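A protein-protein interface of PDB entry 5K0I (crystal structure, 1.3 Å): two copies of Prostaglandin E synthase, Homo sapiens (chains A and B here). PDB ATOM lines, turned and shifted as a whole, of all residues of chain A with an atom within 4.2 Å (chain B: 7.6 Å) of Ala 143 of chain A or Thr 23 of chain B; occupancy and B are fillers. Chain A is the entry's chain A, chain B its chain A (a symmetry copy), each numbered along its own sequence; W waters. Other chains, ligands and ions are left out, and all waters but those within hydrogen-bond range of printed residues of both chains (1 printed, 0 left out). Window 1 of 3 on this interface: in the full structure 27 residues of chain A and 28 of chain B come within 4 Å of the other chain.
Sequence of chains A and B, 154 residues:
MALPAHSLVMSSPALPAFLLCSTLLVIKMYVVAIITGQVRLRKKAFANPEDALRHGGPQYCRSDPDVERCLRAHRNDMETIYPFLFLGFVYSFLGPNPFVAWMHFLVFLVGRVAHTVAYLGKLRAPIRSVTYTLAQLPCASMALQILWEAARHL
Leu 87 of chain A touches Tyr 30 of chain B.
Cys 139 of chain A touches Tyr 30 of chain B (CB to OH, 3.3 Å).
Ala 143 of chain A touches Thr 23 of chain B.
CG2 of Ile 146 of chain A touches OG1 of Thr 23 of chain B (3.2 Å).
Thr 23 of chain B touches Leu 147 of chain A.
Leu 24 of chain B touches Leu 147 of chain A.
Leu 147 of chain A touches Ile 27 of chain B.
No position is printed for both chains.
Of the 7 pairs that touch across the chains among the printed residues, none has its exchanged pair printed and touching as well.
Hydrophobic or aromatic side chains of chain B within 4 Å of the printed part of chain A: Leu 24, Ile 27 and Tyr 30.
Hydrophobic or aromatic side chains of chain A that line the printed part of chain B: Leu 87, Ala 143, Ile 146 and Leu 147.
Among the printed residues, 7 pairs touch across the chains.
Among the printed residues, no Asp or Glu carboxylate lies within 4 Å of a Lys or Arg side-chain nitrogen of the other chain.
Printed residues of chain B within 4 Å of Ala 143 of chain A: Thr 23.
Of the printed residues of chain B, Cys 139 of chain A touches Tyr 30 (3.3 Å).
Of the printed residues of chain B, Leu 147 of chain A touches Thr 23 (3.8 Å), Leu 24 (3.9 Å) and Ile 27 (3.7 Å).
Printed residues of chain A within 4 Å of Tyr 30 of chain B: Leu 87 and Cys 139.
Of the printed residues of chain B, Leu 87 of chain A touches Tyr 30 (3.4 Å).
OG1 of Thr 23 of chain B is in hydrogen-bond range of O of Leu 19 of chain B.
Water W1 bridges OH of Tyr 30 of chain B (2.7 Å) and SG of Cys 139 of chain A (3.4 Å).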
ATOM      1  N   LEU A  87      30.662   8.580  24.633  1.00  0.00           N
ATOM      2  CA  LEU A  87      30.952   9.454  23.497  1.00  0.00           C
ATOM      3  C   LEU A  87      31.831   8.769  22.468  1.00  0.00           C
ATOM      4  O   LEU A  87      31.568   8.858  21.266  1.00  0.00           O
ATOM      5  CB  LEU A  87      31.637  10.738  23.958  1.00  0.00           C
ATOM      6  CG  LEU A  87      30.851  11.704  24.850  1.00  0.00           C
ATOM      7  CD1 LEU A  87      31.785  12.781  25.381  1.00  0.00           C
ATOM      8  CD2 LEU A  87      29.659  12.333  24.132  1.00  0.00           C
ATOM      9  N   CYS A 139      37.096  14.897  24.281  1.00  0.00           N
ATOM     10  CA  CYS A 139      35.714  14.641  24.697  1.00  0.00           C
ATOM     11  C   CYS A 139      34.769  15.742  24.212  1.00  0.00           C
ATOM     12  O   CYS A 139      33.695  15.450  23.684  1.00  0.00           O
ATOM     13  CB  CYS A 139      35.630  14.479  26.216  1.00  0.00           C
ATOM     14  SG  CYS A 139      36.513  13.039  26.824  1.00  0.00           S
ATOM     15  N   ALA A 140      35.183  17.000  24.376  1.00  0.00           N
ATOM     16  CA  ALA A 140      34.402  18.134  23.865  1.00  0.00           C
ATOM     17  C   ALA A 140      34.236  18.035  22.348  1.00  0.00           C
ATOM     18  O   ALA A 140      33.135  18.245  21.815  1.00  0.00           O
ATOM     19  CB  ALA A 140      35.075  19.446  24.242  1.00  0.00           C
ATOM     20  N   SER A 141      35.323  17.681  21.667  1.00  0.00           N
ATOM     21  CA  SER A 141      35.306  17.528  20.213  1.00  0.00           C
ATOM     22  C   SER A 141      34.310  16.455  19.763  1.00  0.00           C
ATOM     23  O   SER A 141      33.486  16.689  18.869  1.00  0.00           O
ATOM     24  CB  SER A 141      36.709  17.205  19.706  1.00  0.00           C
ATOM     25  OG  SER A 141      36.678  16.913  18.312  1.00  0.00           O
ATOM     26  N   MET A 142      34.370  15.281  20.392  1.00  0.00           N
ATOM     27  CA  MET A 142      33.447  14.208  20.041  1.00  0.00           C
ATOM     28  C   MET A 142      32.006  14.580  20.349  1.00  0.00           C
ATOM     29  O   MET A 142      31.113  14.291  19.557  1.00  0.00           O
ATOM     30  CB  MET A 142      33.818  12.911  20.754  1.00  0.00           C
ATOM     31  CG  MET A 142      35.134  12.309  20.263  1.00  0.00           C
ATOM     32  SD  MET A 142      35.513  10.710  21.004  1.00  0.00           S
ATOM     33  CE  MET A 142      35.674  11.122  22.747  1.00  0.00           C
ATOM     34  N   ALA A 143      31.776  15.215  21.499  1.00  0.00           N
ATOM     35  CA  ALA A 143      30.423  15.615  21.884  1.00  0.00           C
ATOM     36  C   ALA A 143      29.800  16.540  20.835  1.00  0.00           C
ATOM     37  O   ALA A 143      28.657  16.343  20.439  1.00  0.00           O
ATOM     38  CB  ALA A 143      30.423  16.278  23.257  1.00  0.00           C
ATOM     39  N   LEU A 144      30.557  17.540  20.386  1.00  0.00           N
ATOM     40  CA  LEU A 144      30.049  18.462  19.366  1.00  0.00           C
ATOM     41  C   LEU A 144      29.746  17.740  18.057  1.00  0.00           C
ATOM     42  O   LEU A 144      28.706  17.979  17.438  1.00  0.00           O
ATOM     43  CB  LEU A 144      31.021  19.624  19.135  1.00  0.00           C
ATOM     44  CG  LEU A 144      31.154  20.617  20.290  1.00  0.00           C
ATOM     45  CD1 LEU A 144      32.244  21.636  20.004  1.00  0.00           C
ATOM     46  CD2 LEU A 144      29.831  21.316  20.591  1.00  0.00           C
ATOM     47  N   GLN A 145      30.634  16.836  17.650  1.00  0.00           N
ATOM     48  CA  GLN A 145      30.416  16.083  16.409  1.00  0.00           C
ATOM     49  C   GLN A 145      29.154  15.236  16.476  1.00  0.00           C
ATOM     50  O   GLN A 145      28.392  15.163  15.508  1.00  0.00           O
ATOM     51  CB  GLN A 145      31.634  15.234  16.057  1.00  0.00           C
ATOM     52  CG  GLN A 145      32.855  16.065  15.667  1.00  0.00           C
ATOM     53  CD  GLN A 145      34.086  15.225  15.390  1.00  0.00           C
ATOM     54  OE1 GLN A 145      34.120  14.447  14.433  1.00  0.00           O
ATOM     55  NE2 GLN A 145      35.112  15.384  16.225  1.00  0.00           N
ATOM     56  N   ILE A 146      28.933  14.589  17.618  1.00  0.00           N
ATOM     57  CA  ILE A 146      27.718  13.804  17.827  1.00  0.00           C
ATOM     58  C   ILE A 146      26.473  14.694  17.781  1.00  0.00           C
ATOM     59  O   ILE A 146      25.462  14.318  17.182  1.00  0.00           O
ATOM     60  CB  ILE A 146      27.773  12.991  19.148  1.00  0.00           C
ATOM     61  CG1 ILE A 146      28.900  11.957  19.080  1.00  0.00           C
ATOM     62  CG2 ILE A 146      26.436  12.300  19.406  1.00  0.00           C
ATOM     63  CD1 ILE A 146      29.302  11.390  20.453  1.00  0.00           C
ATOM     64  N   LEU A 147      26.540  15.863  18.420  1.00  0.00           N
ATOM     65  CA  LEU A 147      25.425  16.813  18.404  1.00  0.00           C
ATOM     66  C   LEU A 147      24.997  17.147  16.987  1.00  0.00           C
ATOM     67  O   LEU A 147      23.808  17.097  16.668  1.00  0.00           O
ATOM     68  CB  LEU A 147      25.784  18.119  19.114  1.00  0.00           C
ATOM     69  CG  LEU A 147      25.744  18.238  20.630  1.00  0.00           C
ATOM     70  CD1 LEU A 147      25.931  19.703  20.999  1.00  0.00           C
ATOM     71  CD2 LEU A 147      24.435  17.706  21.208  1.00  0.00           C
ATOM     72  N   PRO B  16      18.432   9.140  16.721  1.00  0.00           N
ATOM     73  CA  PRO B  16      18.907  10.527  16.688  1.00  0.00           C
ATOM     74  C   PRO B  16      18.451  11.343  17.899  1.00  0.00           C
ATOM     75  O   PRO B  16      19.255  12.072  18.478  1.00  0.00           O
ATOM     76  CB  PRO B  16      18.293  11.079  15.386  1.00  0.00           C
ATOM     77  CG  PRO B  16      18.147   9.880  14.516  1.00  0.00           C
ATOM     78  CD  PRO B  16      17.782   8.755  15.448  1.00  0.00           C
ATOM     79  N   ALA B  17      17.187  11.202  18.286  1.00  0.00           N
ATOM     80  CA  ALA B  17      16.669  11.910  19.452  1.00  0.00           C
ATOM     81  C   ALA B  17      17.399  11.487  20.730  1.00  0.00           C
ATOM     82  O   ALA B  17      17.740  12.331  21.565  1.00  0.00           O
ATOM     83  CB  ALA B  17      15.191  11.663  19.609  1.00  0.00           C
ATOM     84  N   PHE B  18      17.638  10.187  20.871  1.00  0.00           N
ATOM     85  CA  PHE B  18      18.371   9.695  22.035  1.00  0.00           C
ATOM     86  C   PHE B  18      19.781  10.301  22.088  1.00  0.00           C
ATOM     87  O   PHE B  18      20.232  10.766  23.142  1.00  0.00           O
ATOM     88  CB  PHE B  18      18.469   8.173  22.056  1.00  0.00           C
ATOM     89  CG  PHE B  18      19.484   7.675  23.051  1.00  0.00           C
ATOM     90  CD1 PHE B  18      19.227   7.756  24.422  1.00  0.00           C
ATOM     91  CD2 PHE B  18      20.722   7.199  22.623  1.00  0.00           C
ATOM     92  CE1 PHE B  18      20.193   7.347  25.358  1.00  0.00           C
ATOM     93  CE2 PHE B  18      21.690   6.789  23.543  1.00  0.00           C
ATOM     94  CZ  PHE B  18      21.419   6.858  24.911  1.00  0.00           C
ATOM     95  N   LEU B  19      20.485  10.269  20.957  1.00  0.00           N
ATOM     96  CA  LEU B  19      21.859  10.765  20.901  1.00  0.00           C
ATOM     97  C   LEU B  19      21.938  12.267  21.173  1.00  0.00           C
ATOM     98  O   LEU B  19      22.873  12.730  21.831  1.00  0.00           O
ATOM     99  CB  LEU B  19      22.515  10.402  19.565  1.00  0.00           C
ATOM    100  CG  LEU B  19      22.754   8.900  19.361  1.00  0.00           C
ATOM    101  CD1 LEU B  19      23.316   8.664  17.961  1.00  0.00           C
ATOM    102  CD2 LEU B  19      23.672   8.295  20.432  1.00  0.00           C
ATOM    103  N   LEU B  20      20.944  13.020  20.701  1.00  0.00           N
ATOM    104  CA  LEU B  20      20.891  14.457  20.947  1.00  0.00           C
ATOM    105  C   LEU B  20      20.721  14.727  22.439  1.00  0.00           C
ATOM    106  O   LEU B  20      21.489  15.491  23.032  1.00  0.00           O
ATOM    107  CB  LEU B  20      19.743  15.105  20.156  1.00  0.00           C
ATOM    108  CG  LEU B  20      19.636  16.627  20.313  1.00  0.00           C
ATOM    109  CD1 LEU B  20      20.641  17.318  19.415  1.00  0.00           C
ATOM    110  CD2 LEU B  20      18.226  17.107  19.992  1.00  0.00           C
ATOM    111  N   CYS B  21      19.720  14.089  23.045  1.00  0.00           N
ATOM    112  CA  CYS B  21      19.439  14.318  24.463  1.00  0.00           C
ATOM    113  C   CYS B  21      20.593  13.874  25.354  1.00  0.00           C
ATOM    114  O   CYS B  21      20.983  14.586  26.283  1.00  0.00           O
ATOM    115  CB  CYS B  21      18.140  13.623  24.872  1.00  0.00           C
ATOM    116  SG  CYS B  21      16.656  14.374  24.119  1.00  0.00           S
ATOM    117  N   SER B  22      21.153  12.708  25.049  1.00  0.00           N
ATOM    118  CA  SER B  22      22.232  12.146  25.860  1.00  0.00           C
ATOM    119  C   SER B  22      23.522  12.970  25.783  1.00  0.00           C
ATOM    120  O   SER B  22      24.224  13.128  26.784  1.00  0.00           O
ATOM    121  CB  SER B  22      22.496  10.694  25.465  1.00  0.00           C
ATOM    122  OG  SER B  22      22.776  10.584  24.085  1.00  0.00           O
ATOM    123  N   THR B  23      23.836  13.498  24.600  1.00  0.00           N
ATOM    124  CA  THR B  23      25.030  14.316  24.427  1.00  0.00           C
ATOM    125  C   THR B  23      24.851  15.668  25.115  1.00  0.00           C
ATOM    126  O   THR B  23      25.776  16.162  25.754  1.00  0.00           O
ATOM    127  CB  THR B  23      25.410  14.456  22.947  1.00  0.00           C
ATOM    128  OG1 THR B  23      25.559  13.144  22.401  1.00  0.00           O
ATOM    129  CG2 THR B  23      26.726  15.195  22.794  1.00  0.00           C
ATOM    130  N   LEU B  24      23.653  16.240  25.022  1.00  0.00           N
ATOM    131  CA  LEU B  24      23.365  17.465  25.764  1.00  0.00           C
ATOM    132  C   LEU B  24      23.516  17.259  27.273  1.00  0.00           C
ATOM    133  O   LEU B  24      24.026  18.133  27.978  1.00  0.00           O
ATOM    134  CB  LEU B  24      21.972  18.004  25.433  1.00  0.00           C
ATOM    135  CG  LEU B  24      21.808  18.611  24.033  1.00  0.00           C
ATOM    136  CD1 LEU B  24      20.323  18.848  23.739  1.00  0.00           C
ATOM    137  CD2 LEU B  24      22.626  19.892  23.866  1.00  0.00           C
ATOM    138  N   LEU B  25      23.088  16.095  27.767  1.00  0.00           N
ATOM    139  CA  LEU B  25      23.215  15.794  29.192  1.00  0.00           C
ATOM    140  C   LEU B  25      24.665  15.600  29.613  1.00  0.00           C
ATOM    141  O   LEU B  25      25.045  16.024  30.711  1.00  0.00           O
ATOM    142  CB  LEU B  25      22.358  14.580  29.558  1.00  0.00           C
ATOM    143  CG  LEU B  25      20.859  14.880  29.597  1.00  0.00           C
ATOM    144  CD1 LEU B  25      20.058  13.589  29.467  1.00  0.00           C
ATOM    145  CD2 LEU B  25      20.493  15.641  30.858  1.00  0.00           C
ATOM    146  N   VAL B  26      25.476  14.967  28.763  1.00  0.00           N
ATOM    147  CA  VAL B  26      26.910  14.871  29.031  1.00  0.00           C
ATOM    148  C   VAL B  26      27.531  16.276  29.103  1.00  0.00           C
ATOM    149  O   VAL B  26      28.284  16.594  30.034  1.00  0.00           O
ATOM    150  CB  VAL B  26      27.629  13.965  28.013  1.00  0.00           C
ATOM    151  CG1 VAL B  26      29.148  14.072  28.185  1.00  0.00           C
ATOM    152  CG2 VAL B  26      27.181  12.515  28.187  1.00  0.00           C
ATOM    153  N   ILE B  27      27.185  17.133  28.144  1.00  0.00           N
ATOM    154  CA  ILE B  27      27.666  18.515  28.169  1.00  0.00           C
ATOM    155  C   ILE B  27      27.214  19.244  29.446  1.00  0.00           C
ATOM    156  O   ILE B  27      27.991  19.972  30.053  1.00  0.00           O
ATOM    157  CB  ILE B  27      27.262  19.277  26.890  1.00  0.00           C
ATOM    158  CG1 ILE B  27      27.983  18.678  25.672  1.00  0.00           C
ATOM    159  CG2 ILE B  27      27.557  20.782  27.046  1.00  0.00           C
ATOM    160  CD1 ILE B  27      27.391  19.096  24.322  1.00  0.00           C
ATOM    161  N   LYS B  28      25.976  18.994  29.869  1.00  0.00           N
ATOM    162  CA  LYS B  28      25.451  19.559  31.111  1.00  0.00           C
ATOM    163  C   LYS B  28      26.240  19.102  32.351  1.00  0.00           C
ATOM    164  O   LYS B  28      26.392  19.872  33.310  1.00  0.00           O
ATOM    165  CB  LYS B  28      23.965  19.226  31.242  1.00  0.00           C
ATOM    166  CG  LYS B  28      23.255  19.922  32.417  1.00  0.00           C
ATOM    167  CD  LYS B  28      22.402  18.916  33.192  1.00  0.00           C
ATOM    168  CE  LYS B  28      23.258  17.916  33.975  1.00  0.00           C
ATOM    169  NZ  LYS B  28      23.990  18.568  35.112  1.00  0.00           N
ATOM    170  N   MET B  29      26.731  17.861  32.332  1.00  0.00           N
ATOM    171  CA  MET B  29      27.609  17.375  33.403  1.00  0.00           C
ATOM    172  C   MET B  29      28.959  18.091  33.368  1.00  0.00           C
ATOM    173  O   MET B  29      29.490  18.488  34.409  1.00  0.00           O
ATOM    174  CB  MET B  29      27.779  15.860  33.316  1.00  0.00           C
ATOM    175  CG  MET B  29      26.457  15.121  33.466  1.00  0.00           C
ATOM    176  SD  MET B  29      26.621  13.330  33.589  1.00  0.00           S
ATOM    177  CE  MET B  29      27.672  13.209  35.040  1.00  0.00           C
ATOM    178  N   TYR B  30      29.497  18.288  32.164  1.00  0.00           N
ATOM    179  CA  TYR B  30      30.740  19.036  31.983  1.00  0.00           C
ATOM    180  C   TYR B  30      30.594  20.472  32.516  1.00  0.00           C
ATOM    181  O   TYR B  30      31.515  21.004  33.146  1.00  0.00           O
ATOM    182  CB  TYR B  30      31.140  19.069  30.507  1.00  0.00           C
ATOM    183  CG  TYR B  30      31.604  17.749  29.928  1.00  0.00           C
ATOM    184  CD1 TYR B  30      31.980  16.676  30.744  1.00  0.00           C
ATOM    185  CD2 TYR B  30      31.716  17.593  28.549  1.00  0.00           C
ATOM    186  CE1 TYR B  30      32.436  15.472  30.187  1.00  0.00           C
ATOM    187  CE2 TYR B  30      32.166  16.411  27.989  1.00  0.00           C
ATOM    188  CZ  TYR B  30      32.526  15.354  28.812  1.00  0.00           C
ATOM    189  OH  TYR B  30      32.980  14.188  28.235  1.00  0.00           O
ATOM    190  N   PHE B  84      20.755   6.303  32.402  1.00  0.00           N
ATOM    191  CA  PHE B  84      20.006   6.717  31.215  1.00  0.00           C
ATOM    192  C   PHE B  84      20.774   6.466  29.918  1.00  0.00           C
ATOM    193  O   PHE B  84      20.182   6.057  28.908  1.00  0.00           O
ATOM    194  CB  PHE B  84      19.630   8.191  31.315  1.00  0.00           C
ATOM    195  CG  PHE B  84      18.962   8.734  30.071  1.00  0.00           C
ATOM    196  CD1 PHE B  84      17.590   8.573  29.868  1.00  0.00           C
ATOM    197  CD2 PHE B  84      19.705   9.417  29.116  1.00  0.00           C
ATOM    198  CE1 PHE B  84      16.972   9.088  28.722  1.00  0.00           C
ATOM    199  CE2 PHE B  84      19.095   9.925  27.966  1.00  0.00           C
ATOM    200  CZ  PHE B  84      17.729   9.763  27.773  1.00  0.00           C
ATOM    201  N   LEU B  85      22.084   6.706  29.931  1.00  0.00           N
ATOM    202  CA  LEU B  85      22.894   6.500  28.729  1.00  0.00           C
ATOM    203  C   LEU B  85      22.813   5.050  28.284  1.00  0.00           C
ATOM    204  O   LEU B  85      22.765   4.761  27.092  1.00  0.00           O
ATOM    205  CB  LEU B  85      24.346   6.902  28.963  1.00  0.00           C
ATOM    206  CG  LEU B  85      24.636   8.373  29.273  1.00  0.00           C
ATOM    207  CD1 LEU B  85      26.120   8.587  29.540  1.00  0.00           C
ATOM    208  CD2 LEU B  85      24.169   9.290  28.153  1.00  0.00           C
ATOM    209  N   LEU B 109      15.580  14.745  29.819  1.00  0.00           N
ATOM    210  CA  LEU B 109      16.416  15.915  29.572  1.00  0.00           C
ATOM    211  C   LEU B 109      15.946  17.133  30.363  1.00  0.00           C
ATOM    212  O   LEU B 109      16.743  17.767  31.059  1.00  0.00           O
ATOM    213  CB  LEU B 109      16.459  16.234  28.076  1.00  0.00           C
ATOM    214  CG  LEU B 109      17.168  17.527  27.643  1.00  0.00           C
ATOM    215  CD1 LEU B 109      18.657  17.492  27.955  1.00  0.00           C
ATOM    216  CD2 LEU B 109      16.924  17.777  26.152  1.00  0.00           C
HETATM  217  O   HOH W   1      34.908  13.134  29.805  1.00  0.00           O
